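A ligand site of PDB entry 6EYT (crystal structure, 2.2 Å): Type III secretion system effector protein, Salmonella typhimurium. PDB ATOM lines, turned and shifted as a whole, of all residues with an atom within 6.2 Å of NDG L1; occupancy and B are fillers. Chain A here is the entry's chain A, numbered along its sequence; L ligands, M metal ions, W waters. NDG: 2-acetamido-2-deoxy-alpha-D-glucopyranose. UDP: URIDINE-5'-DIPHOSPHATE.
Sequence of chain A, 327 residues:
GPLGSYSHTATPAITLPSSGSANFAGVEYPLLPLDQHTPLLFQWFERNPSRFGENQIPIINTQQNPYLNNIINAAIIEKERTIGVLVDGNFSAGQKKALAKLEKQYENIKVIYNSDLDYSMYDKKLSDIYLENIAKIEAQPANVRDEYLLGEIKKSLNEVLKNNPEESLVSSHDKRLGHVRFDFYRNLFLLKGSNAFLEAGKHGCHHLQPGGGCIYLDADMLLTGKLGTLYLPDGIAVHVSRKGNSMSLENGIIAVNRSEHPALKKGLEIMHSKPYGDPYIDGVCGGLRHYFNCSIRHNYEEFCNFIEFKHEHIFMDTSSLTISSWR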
ATOM      1  N   HIS A 179       3.240  36.021  -2.794  1.00  0.00           N
ATOM      2  CA  HIS A 179       3.885  34.746  -3.040  1.00  0.00           C
ATOM      3  C   HIS A 179       5.379  34.912  -3.284  1.00  0.00           C
ATOM      4  O   HIS A 179       6.181  34.092  -2.843  1.00  0.00           O
ATOM      5  CB  HIS A 179       3.228  34.047  -4.225  1.00  0.00           C
ATOM      6  CG  HIS A 179       3.531  34.671  -5.539  1.00  0.00           C
ATOM      7  ND1 HIS A 179       2.980  35.877  -5.933  1.00  0.00           N
ATOM      8  CD2 HIS A 179       4.352  34.285  -6.543  1.00  0.00           C
ATOM      9  CE1 HIS A 179       3.431  36.195  -7.131  1.00  0.00           C
ATOM     10  NE2 HIS A 179       4.267  35.250  -7.522  1.00  0.00           N
ATOM     11  N   PHE A 182       7.011  34.891   0.232  1.00  0.00           N
ATOM     12  CA  PHE A 182       7.029  33.648   0.981  1.00  0.00           C
ATOM     13  C   PHE A 182       7.618  32.498   0.175  1.00  0.00           C
ATOM     14  O   PHE A 182       8.180  31.569   0.761  1.00  0.00           O
ATOM     15  CB  PHE A 182       5.646  33.302   1.568  1.00  0.00           C
ATOM     16  CG  PHE A 182       4.524  33.182   0.579  1.00  0.00           C
ATOM     17  CD1 PHE A 182       4.383  32.046  -0.211  1.00  0.00           C
ATOM     18  CD2 PHE A 182       3.510  34.136   0.559  1.00  0.00           C
ATOM     19  CE1 PHE A 182       3.297  31.917  -1.072  1.00  0.00           C
ATOM     20  CE2 PHE A 182       2.433  34.010  -0.291  1.00  0.00           C
ATOM     21  CZ  PHE A 182       2.320  32.902  -1.116  1.00  0.00           C
ATOM     22  N   ASP A 183       7.550  32.563  -1.158  1.00  0.00           N
ATOM     23  CA  ASP A 183       8.332  31.601  -1.955  1.00  0.00           C
ATOM     24  C   ASP A 183       9.810  31.727  -1.632  1.00  0.00           C
ATOM     25  O   ASP A 183      10.524  30.722  -1.531  1.00  0.00           O
ATOM     26  CB  ASP A 183       8.115  31.849  -3.450  1.00  0.00           C
ATOM     27  CG  ASP A 183       6.850  31.198  -3.986  1.00  0.00           C
ATOM     28  OD1 ASP A 183       6.202  30.428  -3.244  1.00  0.00           O
ATOM     29  OD2 ASP A 183       6.523  31.440  -5.173  1.00  0.00           O
ATOM     30  N   ARG A 186      10.695  30.327   1.759  1.00  0.00           N
ATOM     31  CA  ARG A 186      10.525  28.873   1.778  1.00  0.00           C
ATOM     32  C   ARG A 186      11.818  28.192   1.358  1.00  0.00           C
ATOM     33  O   ARG A 186      12.251  27.226   1.994  1.00  0.00           O
ATOM     34  CB  ARG A 186       9.371  28.469   0.864  1.00  0.00           C
ATOM     35  CG  ARG A 186       9.058  26.965   0.831  1.00  0.00           C
ATOM     36  CD  ARG A 186       7.948  26.666  -0.167  1.00  0.00           C
ATOM     37  NE  ARG A 186       6.756  27.463   0.113  1.00  0.00           N
ATOM     38  CZ  ARG A 186       5.735  27.595  -0.726  1.00  0.00           C
ATOM     39  NH1 ARG A 186       5.736  26.974  -1.904  1.00  0.00           N
ATOM     40  NH2 ARG A 186       4.691  28.347  -0.378  1.00  0.00           N
ATOM     41  N   TYR A 216       8.660  20.011   3.047  1.00  0.00           N
ATOM     42  CA  TYR A 216       7.724  21.124   2.972  1.00  0.00           C
ATOM     43  C   TYR A 216       6.464  20.725   2.220  1.00  0.00           C
ATOM     44  O   TYR A 216       6.535  20.070   1.177  1.00  0.00           O
ATOM     45  CB  TYR A 216       8.335  22.351   2.289  1.00  0.00           C
ATOM     46  CG  TYR A 216       7.243  23.340   2.014  1.00  0.00           C
ATOM     47  CD1 TYR A 216       6.806  24.198   3.004  1.00  0.00           C
ATOM     48  CD2 TYR A 216       6.587  23.360   0.784  1.00  0.00           C
ATOM     49  CE1 TYR A 216       5.770  25.085   2.781  1.00  0.00           C
ATOM     50  CE2 TYR A 216       5.545  24.238   0.559  1.00  0.00           C
ATOM     51  CZ  TYR A 216       5.147  25.104   1.561  1.00  0.00           C
ATOM     52  OH  TYR A 216       4.116  25.974   1.339  1.00  0.00           O
ATOM     53  N   ASP A 218       2.474  22.333   1.008  1.00  0.00           N
ATOM     54  CA  ASP A 218       1.433  23.345   1.021  1.00  0.00           C
ATOM     55  C   ASP A 218       0.339  22.912   1.985  1.00  0.00           C
ATOM     56  O   ASP A 218       0.032  21.713   2.101  1.00  0.00           O
ATOM     57  CB  ASP A 218       0.874  23.559  -0.388  1.00  0.00           C
ATOM     58  CG  ASP A 218       1.616  24.621  -1.164  1.00  0.00           C
ATOM     59  OD1 ASP A 218       2.520  25.260  -0.584  1.00  0.00           O
ATOM     60  OD2 ASP A 218       1.316  24.812  -2.369  1.00  0.00           O
ATOM     61  N   ASP A 220      -2.631  22.922   1.795  1.00  0.00           N
ATOM     62  CA  ASP A 220      -3.713  22.202   1.137  1.00  0.00           C
ATOM     63  C   ASP A 220      -3.284  20.822   0.630  1.00  0.00           C
ATOM     64  O   ASP A 220      -4.080  20.162  -0.061  1.00  0.00           O
ATOM     65  CB  ASP A 220      -4.277  23.036  -0.024  1.00  0.00           C
ATOM     66  CG  ASP A 220      -3.323  23.092  -1.216  1.00  0.00           C
ATOM     67  OD1 ASP A 220      -2.201  22.548  -1.144  1.00  0.00           O
ATOM     68  OD2 ASP A 220      -3.704  23.699  -2.231  1.00  0.00           O
ATOM     69  N   MET A 221      -2.076  20.375   0.954  1.00  0.00           N
ATOM     70  CA  MET A 221      -1.616  19.012   0.678  1.00  0.00           C
ATOM     71  C   MET A 221      -2.074  18.160   1.844  1.00  0.00           C
ATOM     72  O   MET A 221      -1.431  18.143   2.908  1.00  0.00           O
ATOM     73  CB  MET A 221      -0.092  18.971   0.524  1.00  0.00           C
ATOM     74  CG  MET A 221       0.491  19.867  -0.573  1.00  0.00           C
ATOM     75  SD  MET A 221       0.321  19.242  -2.271  1.00  0.00           S
ATOM     76  CE  MET A 221       0.860  20.669  -3.240  1.00  0.00           C
ATOM     77  N   HIS A 239       7.038  18.706  -5.950  1.00  0.00           N
ATOM     78  CA  HIS A 239       5.738  18.511  -6.567  1.00  0.00           C
ATOM     79  C   HIS A 239       5.846  18.674  -8.071  1.00  0.00           C
ATOM     80  O   HIS A 239       6.596  19.509  -8.574  1.00  0.00           O
ATOM     81  CB  HIS A 239       4.742  19.529  -5.988  1.00  0.00           C
ATOM     82  CG  HIS A 239       3.352  19.397  -6.515  1.00  0.00           C
ATOM     83  ND1 HIS A 239       2.679  18.197  -6.569  1.00  0.00           N
ATOM     84  CD2 HIS A 239       2.489  20.329  -6.988  1.00  0.00           C
ATOM     85  CE1 HIS A 239       1.473  18.390  -7.066  1.00  0.00           C
ATOM     86  NE2 HIS A 239       1.330  19.677  -7.324  1.00  0.00           N
ATOM     87  N   SER A 241       2.978  19.219 -10.912  1.00  0.00           N
ATOM     88  CA  SER A 241       1.553  19.425 -11.079  1.00  0.00           C
ATOM     89  C   SER A 241       1.140  19.079 -12.494  1.00  0.00           C
ATOM     90  O   SER A 241       1.903  19.228 -13.447  1.00  0.00           O
ATOM     91  CB  SER A 241       1.165  20.875 -10.799  1.00  0.00           C
ATOM     92  OG  SER A 241       1.465  21.686 -11.916  1.00  0.00           O
ATOM     93  N   GLU A 250       6.841  22.130  -9.527  1.00  0.00           N
ATOM     94  CA  GLU A 250       6.168  23.052  -8.628  1.00  0.00           C
ATOM     95  C   GLU A 250       6.940  23.092  -7.317  1.00  0.00           C
ATOM     96  O   GLU A 250       7.770  22.222  -7.041  1.00  0.00           O
ATOM     97  CB  GLU A 250       4.708  22.641  -8.392  1.00  0.00           C
ATOM     98  CG  GLU A 250       3.744  23.227  -9.404  1.00  0.00           C
ATOM     99  CD  GLU A 250       3.799  24.745  -9.457  1.00  0.00           C
ATOM    100  OE1 GLU A 250       4.450  25.367  -8.574  1.00  0.00           O
ATOM    101  OE2 GLU A 250       3.191  25.313 -10.392  1.00  0.00           O
ATOM    102  N   ASN A 251       6.691  24.119  -6.512  1.00  0.00           N
ATOM    103  CA  ASN A 251       7.299  24.219  -5.192  1.00  0.00           C
ATOM    104  C   ASN A 251       6.279  24.004  -4.074  1.00  0.00           C
ATOM    105  O   ASN A 251       6.560  24.312  -2.920  1.00  0.00           O
ATOM    106  CB  ASN A 251       8.029  25.558  -5.009  1.00  0.00           C
ATOM    107  CG  ASN A 251       7.110  26.755  -5.118  1.00  0.00           C
ATOM    108  OD1 ASN A 251       6.008  26.660  -5.642  1.00  0.00           O
ATOM    109  ND2 ASN A 251       7.560  27.891  -4.616  1.00  0.00           N
ATOM    110  N   GLY A 252       5.086  23.499  -4.410  1.00  0.00           N
ATOM    111  CA  GLY A 252       4.097  23.145  -3.411  1.00  0.00           C
ATOM    112  C   GLY A 252       4.513  21.998  -2.513  1.00  0.00           C
ATOM    113  O   GLY A 252       3.987  21.865  -1.396  1.00  0.00           O
ATOM    114  N   ILE A 253       5.420  21.147  -2.979  1.00  0.00           N
ATOM    115  CA  ILE A 253       6.078  20.148  -2.142  1.00  0.00           C
ATOM    116  C   ILE A 253       7.561  20.193  -2.464  1.00  0.00           C
ATOM    117  O   ILE A 253       7.943  20.116  -3.636  1.00  0.00           O
ATOM    118  CB  ILE A 253       5.567  18.711  -2.381  1.00  0.00           C
ATOM    119  CG1 ILE A 253       4.067  18.605  -2.112  1.00  0.00           C
ATOM    120  CG2 ILE A 253       6.341  17.734  -1.510  1.00  0.00           C
ATOM    121  CD1 ILE A 253       3.510  17.262  -2.586  1.00  0.00           C
ATOM    122  N   ASP A 278      13.883  34.868  -9.856  1.00  0.00           N
ATOM    123  CA  ASP A 278      12.612  34.494  -9.262  1.00  0.00           C
ATOM    124  C   ASP A 278      12.815  33.344  -8.269  1.00  0.00           C
ATOM    125  O   ASP A 278      13.387  32.303  -8.645  1.00  0.00           O
ATOM    126  CB  ASP A 278      11.628  34.083 -10.357  1.00  0.00           C
ATOM    127  CG  ASP A 278      10.268  33.707  -9.810  1.00  0.00           C
ATOM    128  OD1 ASP A 278       9.484  34.627  -9.458  1.00  0.00           O
ATOM    129  OD2 ASP A 278       9.974  32.499  -9.743  1.00  0.00           O
ATOM    130  N   TYR A 280      10.879  31.043  -7.359  1.00  0.00           N
ATOM    131  CA  TYR A 280      10.295  29.801  -7.862  1.00  0.00           C
ATOM    132  C   TYR A 280      10.974  29.340  -9.154  1.00  0.00           C
ATOM    133  O   TYR A 280      11.511  28.228  -9.220  1.00  0.00           O
ATOM    134  CB  TYR A 280       8.782  29.987  -8.099  1.00  0.00           C
ATOM    135  CG  TYR A 280       8.189  28.915  -8.983  1.00  0.00           C
ATOM    136  CD1 TYR A 280       8.296  27.570  -8.643  1.00  0.00           C
ATOM    137  CD2 TYR A 280       7.529  29.247 -10.155  1.00  0.00           C
ATOM    138  CE1 TYR A 280       7.752  26.578  -9.441  1.00  0.00           C
ATOM    139  CE2 TYR A 280       6.975  28.251 -10.964  1.00  0.00           C
ATOM    140  CZ  TYR A 280       7.095  26.929 -10.603  1.00  0.00           C
ATOM    141  OH  TYR A 280       6.553  25.949 -11.408  1.00  0.00           O
ATOM    142  N   ASP A 317      -2.646  19.583  -3.622  1.00  0.00           N
ATOM    143  CA  ASP A 317      -3.175  20.861  -4.109  1.00  0.00           C
ATOM    144  C   ASP A 317      -4.705  20.896  -4.104  1.00  0.00           C
ATOM    145  O   ASP A 317      -5.355  21.155  -5.124  1.00  0.00           O
ATOM    146  CB  ASP A 317      -2.631  21.181  -5.509  1.00  0.00           C
ATOM    147  CG  ASP A 317      -2.947  22.617  -5.975  1.00  0.00           C
ATOM    148  OD1 ASP A 317      -3.178  23.494  -5.117  1.00  0.00           O
ATOM    149  OD2 ASP A 317      -2.942  22.875  -7.193  1.00  0.00           O
ATOM    150  N   TRP A 326      -4.513  33.015  -2.191  1.00  0.00           N
ATOM    151  CA  TRP A 326      -3.857  34.285  -2.498  1.00  0.00           C
ATOM    152  C   TRP A 326      -4.012  34.751  -3.945  1.00  0.00           C
ATOM    153  O   TRP A 326      -3.715  35.925  -4.220  1.00  0.00           O
ATOM    154  CB  TRP A 326      -2.358  34.199  -2.184  1.00  0.00           C
ATOM    155  CG  TRP A 326      -1.635  33.216  -3.028  1.00  0.00           C
ATOM    156  CD1 TRP A 326      -1.502  31.870  -2.799  1.00  0.00           C
ATOM    157  CD2 TRP A 326      -0.924  33.482  -4.238  1.00  0.00           C
ATOM    158  NE1 TRP A 326      -0.747  31.290  -3.797  1.00  0.00           N
ATOM    159  CE2 TRP A 326      -0.392  32.267  -4.696  1.00  0.00           C
ATOM    160  CE3 TRP A 326      -0.699  34.644  -4.983  1.00  0.00           C
ATOM    161  CZ2 TRP A 326       0.365  32.177  -5.858  1.00  0.00           C
ATOM    162  CZ3 TRP A 326       0.045  34.550  -6.142  1.00  0.00           C
ATOM    163  CH2 TRP A 326       0.573  33.328  -6.565  1.00  0.00           C
ATOM    164  N   ARG A 327      -4.438  33.899  -4.876  1.00  0.00           N
ATOM    165  CA  ARG A 327      -4.607  34.337  -6.271  1.00  0.00           C
ATOM    166  C   ARG A 327      -5.952  35.015  -6.499  1.00  0.00           C
ATOM    167  O   ARG A 327      -6.908  34.813  -5.738  1.00  0.00           O
ATOM    168  CB  ARG A 327      -4.464  33.153  -7.242  1.00  0.00           C
ATOM    169  CG  ARG A 327      -3.126  32.440  -7.143  1.00  0.00           C
ATOM    170  CD  ARG A 327      -3.089  31.227  -8.058  1.00  0.00           C
ATOM    171  NE  ARG A 327      -1.925  30.379  -7.796  1.00  0.00           N
ATOM    172  CZ  ARG A 327      -0.788  30.438  -8.487  1.00  0.00           C
ATOM    173  NH1 ARG A 327      -0.670  31.306  -9.490  1.00  0.00           N
ATOM    174  NH2 ARG A 327       0.216  29.640  -8.186  1.00  0.00           N
HETATM  175  C1  NDG L   1       2.357  27.177  -6.769  1.00  0.00           C
HETATM  176  C2  NDG L   1       2.578  26.432  -5.426  1.00  0.00           C
HETATM  177  C3  NDG L   1       2.580  27.421  -4.236  1.00  0.00           C
HETATM  178  C4  NDG L   1       3.518  28.598  -4.551  1.00  0.00           C
HETATM  179  C5  NDG L   1       3.026  29.289  -5.827  1.00  0.00           C
HETATM  180  C6  NDG L   1       3.831  30.529  -6.219  1.00  0.00           C
HETATM  181  C7  NDG L   1       1.740  24.111  -5.842  1.00  0.00           C
HETATM  182  C8  NDG L   1       0.585  23.126  -5.641  1.00  0.00           C
HETATM  183  O5  NDG L   1       3.184  28.346  -6.902  1.00  0.00           O
HETATM  184  O3  NDG L   1       3.006  26.772  -3.042  1.00  0.00           O
HETATM  185  O4  NDG L   1       3.563  29.490  -3.437  1.00  0.00           O
HETATM  186  O6  NDG L   1       5.141  30.187  -6.698  1.00  0.00           O
HETATM  187  O7  NDG L   1       2.750  23.768  -6.472  1.00  0.00           O
HETATM  188  N2  NDG L   1       1.585  25.366  -5.296  1.00  0.00           N
HETATM  189  O1  NDG L   1       0.997  27.511  -6.879  1.00  0.00           O
HETATM  190  N1  UDP L   2       0.542  31.114   1.570  1.00  0.00           N
HETATM  191  C2  UDP L   2       0.921  31.934   2.603  1.00  0.00           C
HETATM  192  N3  UDP L   2       0.133  33.038   2.790  1.00  0.00           N
HETATM  193  C4  UDP L   2      -0.978  33.403   2.053  1.00  0.00           C
HETATM  194  C5  UDP L   2      -1.318  32.499   1.002  1.00  0.00           C
HETATM  195  C6  UDP L   2      -0.554  31.405   0.794  1.00  0.00           C
HETATM  196  O2  UDP L   2       1.886  31.713   3.317  1.00  0.00           O
HETATM  197  O4  UDP L   2      -1.600  34.438   2.348  1.00  0.00           O
HETATM  198  C1' UDP L   2       1.344  29.905   1.327  1.00  0.00           C
HETATM  199  C2' UDP L   2       0.950  28.739   2.246  1.00  0.00           C
HETATM  200  O2' UDP L   2       2.109  28.014   2.618  1.00  0.00           O
HETATM  201  C3' UDP L   2       0.073  27.886   1.319  1.00  0.00           C
HETATM  202  C4' UDP L   2       0.775  28.079  -0.015  1.00  0.00           C
HETATM  203  O4' UDP L   2       1.154  29.483  -0.008  1.00  0.00           O
HETATM  204  O3' UDP L   2       0.085  26.528   1.720  1.00  0.00           O
HETATM  205  C5' UDP L   2      -0.049  27.780  -1.242  1.00  0.00           C
HETATM  206  O5' UDP L   2      -1.416  28.199  -1.002  1.00  0.00           O
HETATM  207  PA  UDP L   2      -2.579  27.839  -2.011  1.00  0.00           P
HETATM  208  O1A UDP L   2      -2.537  26.360  -2.214  1.00  0.00           O
HETATM  209  O2A UDP L   2      -3.913  28.440  -1.557  1.00  0.00           O
HETATM  210  O3A UDP L   2      -2.190  28.590  -3.365  1.00  0.00           O
HETATM  211  PB  UDP L   2      -1.997  27.930  -4.801  1.00  0.00           P
HETATM  212  O1B UDP L   2      -2.012  26.456  -4.740  1.00  0.00           O
HETATM  213  O2B UDP L   2      -0.654  28.509  -5.272  1.00  0.00           O
HETATM  214  O3B UDP L   2      -3.132  28.542  -5.608  1.00  0.00           O
HETATM  215 MN    MN M   1      -2.904  25.008  -3.710  1.00  0.00          MN
HETATM  216  O   HOH W   1      -1.052  23.714  -3.322  1.00  0.00           O
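An oxygen (O6) of NDG L1 is in hydrogen-bond range of the side-chain carboxylate (OD2) of Asp 183 (2.4 Å).
The guanidinium group (NH2) of Arg 327 sits at hydrogen-bond distance from an oxygen (O1) of NDG L1, 2.6 Å away.
The side-chain carboxylate (OD2) of Asp 218 is in hydrogen-bond range of an oxygen (O3) of NDG L1 (2.7 Å).
The guanidinium group of Arg 186 lies within hydrogen-bond range of an oxygen (O3) of NDG L1, at 3.0 Å.
The backbone NH of Gly 252 lies within hydrogen-bond range of an oxygen (O7) of NDG L1, 3.1 Å away.
An oxygen (O3B) of UDP L2 lies within salt-bridge range of the guanidinium group (NE) of Arg 327 (3.1 Å).
The indole nitrogen (NE1) of Trp 326 is in hydrogen-bond range of an oxygen (O3A) of UDP L2.
O2' of UDP L2 is in hydrogen-bond range of OH of Tyr 216.
O1 of NDG L1 is in hydrogen-bond range of O2B of UDP L2, 2.5 Å away.
NH1 of Arg 186 is in salt-bridge range of OD1 of Asp 183 (3.7 Å).
The side-chain carboxylate (OD1) of Asp 183 lies within hydrogen-bond range of the side-chain amide nitrogen (ND2) of Asn 251 (3.2 Å).
The side-chain carboxylate (OD1) of Asp 218 is in salt-bridge range of the guanidinium group (NH2) of Arg 186 (3.8 Å).
The backbone NH (N) of Asp 218 is in hydrogen-bond range of the backbone carbonyl oxygen (O) of Gly 252, at 2.9 Å.
The backbone carbonyl oxygen of Asn 251 is in hydrogen-bond range of the guanidinium group of Arg 186, at 3.0 Å.
OH of Tyr 216 is in hydrogen-bond range of NH2 of Arg 186 (3.0 Å).
SD of Met 221 sits at hydrogen-bond distance from N of Asp 317, at 3.3 Å.
N of Tyr 280 sits at hydrogen-bond distance from OD2 of Asp 278 (2.9 Å).
OE1 of Glu 250 lies close to O7 of NDG L1 (3.1 Å).
CD2 of His 179 touches C6 of NDG L1 (3.8 Å).
Phe 182 touches NDG L1.
Met 221 touches NDG L1.
His 239 touches NDG L1 (CD2 to O7, 3.5 Å).
Asn 251 touches NDG L1.
Tyr 280 touches NDG L1.
Asp 317 touches NDG L1.
Trp 326 touches NDG L1.
Hydrophobic or aromatic side chains that line NDG L1: His 179, Phe 182, Met 221, His 239, Tyr 280 and Trp 326.
14 residues have an atom within 4 Å of NDG L1: His 179, Phe 182, Asp 183, Arg 186, Asp 218, Met 221, His 239, Glu 250, Asn 251, Gly 252, Tyr 280, Asp 317, Trp 326 and Arg 327.
Water W1 lies within hydrogen-bond range of the side-chain carboxylate (OD1) of Asp 220 (2.7 Å) and the side-chain carboxylate (OD2) of Asp 218 (2.8 Å).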
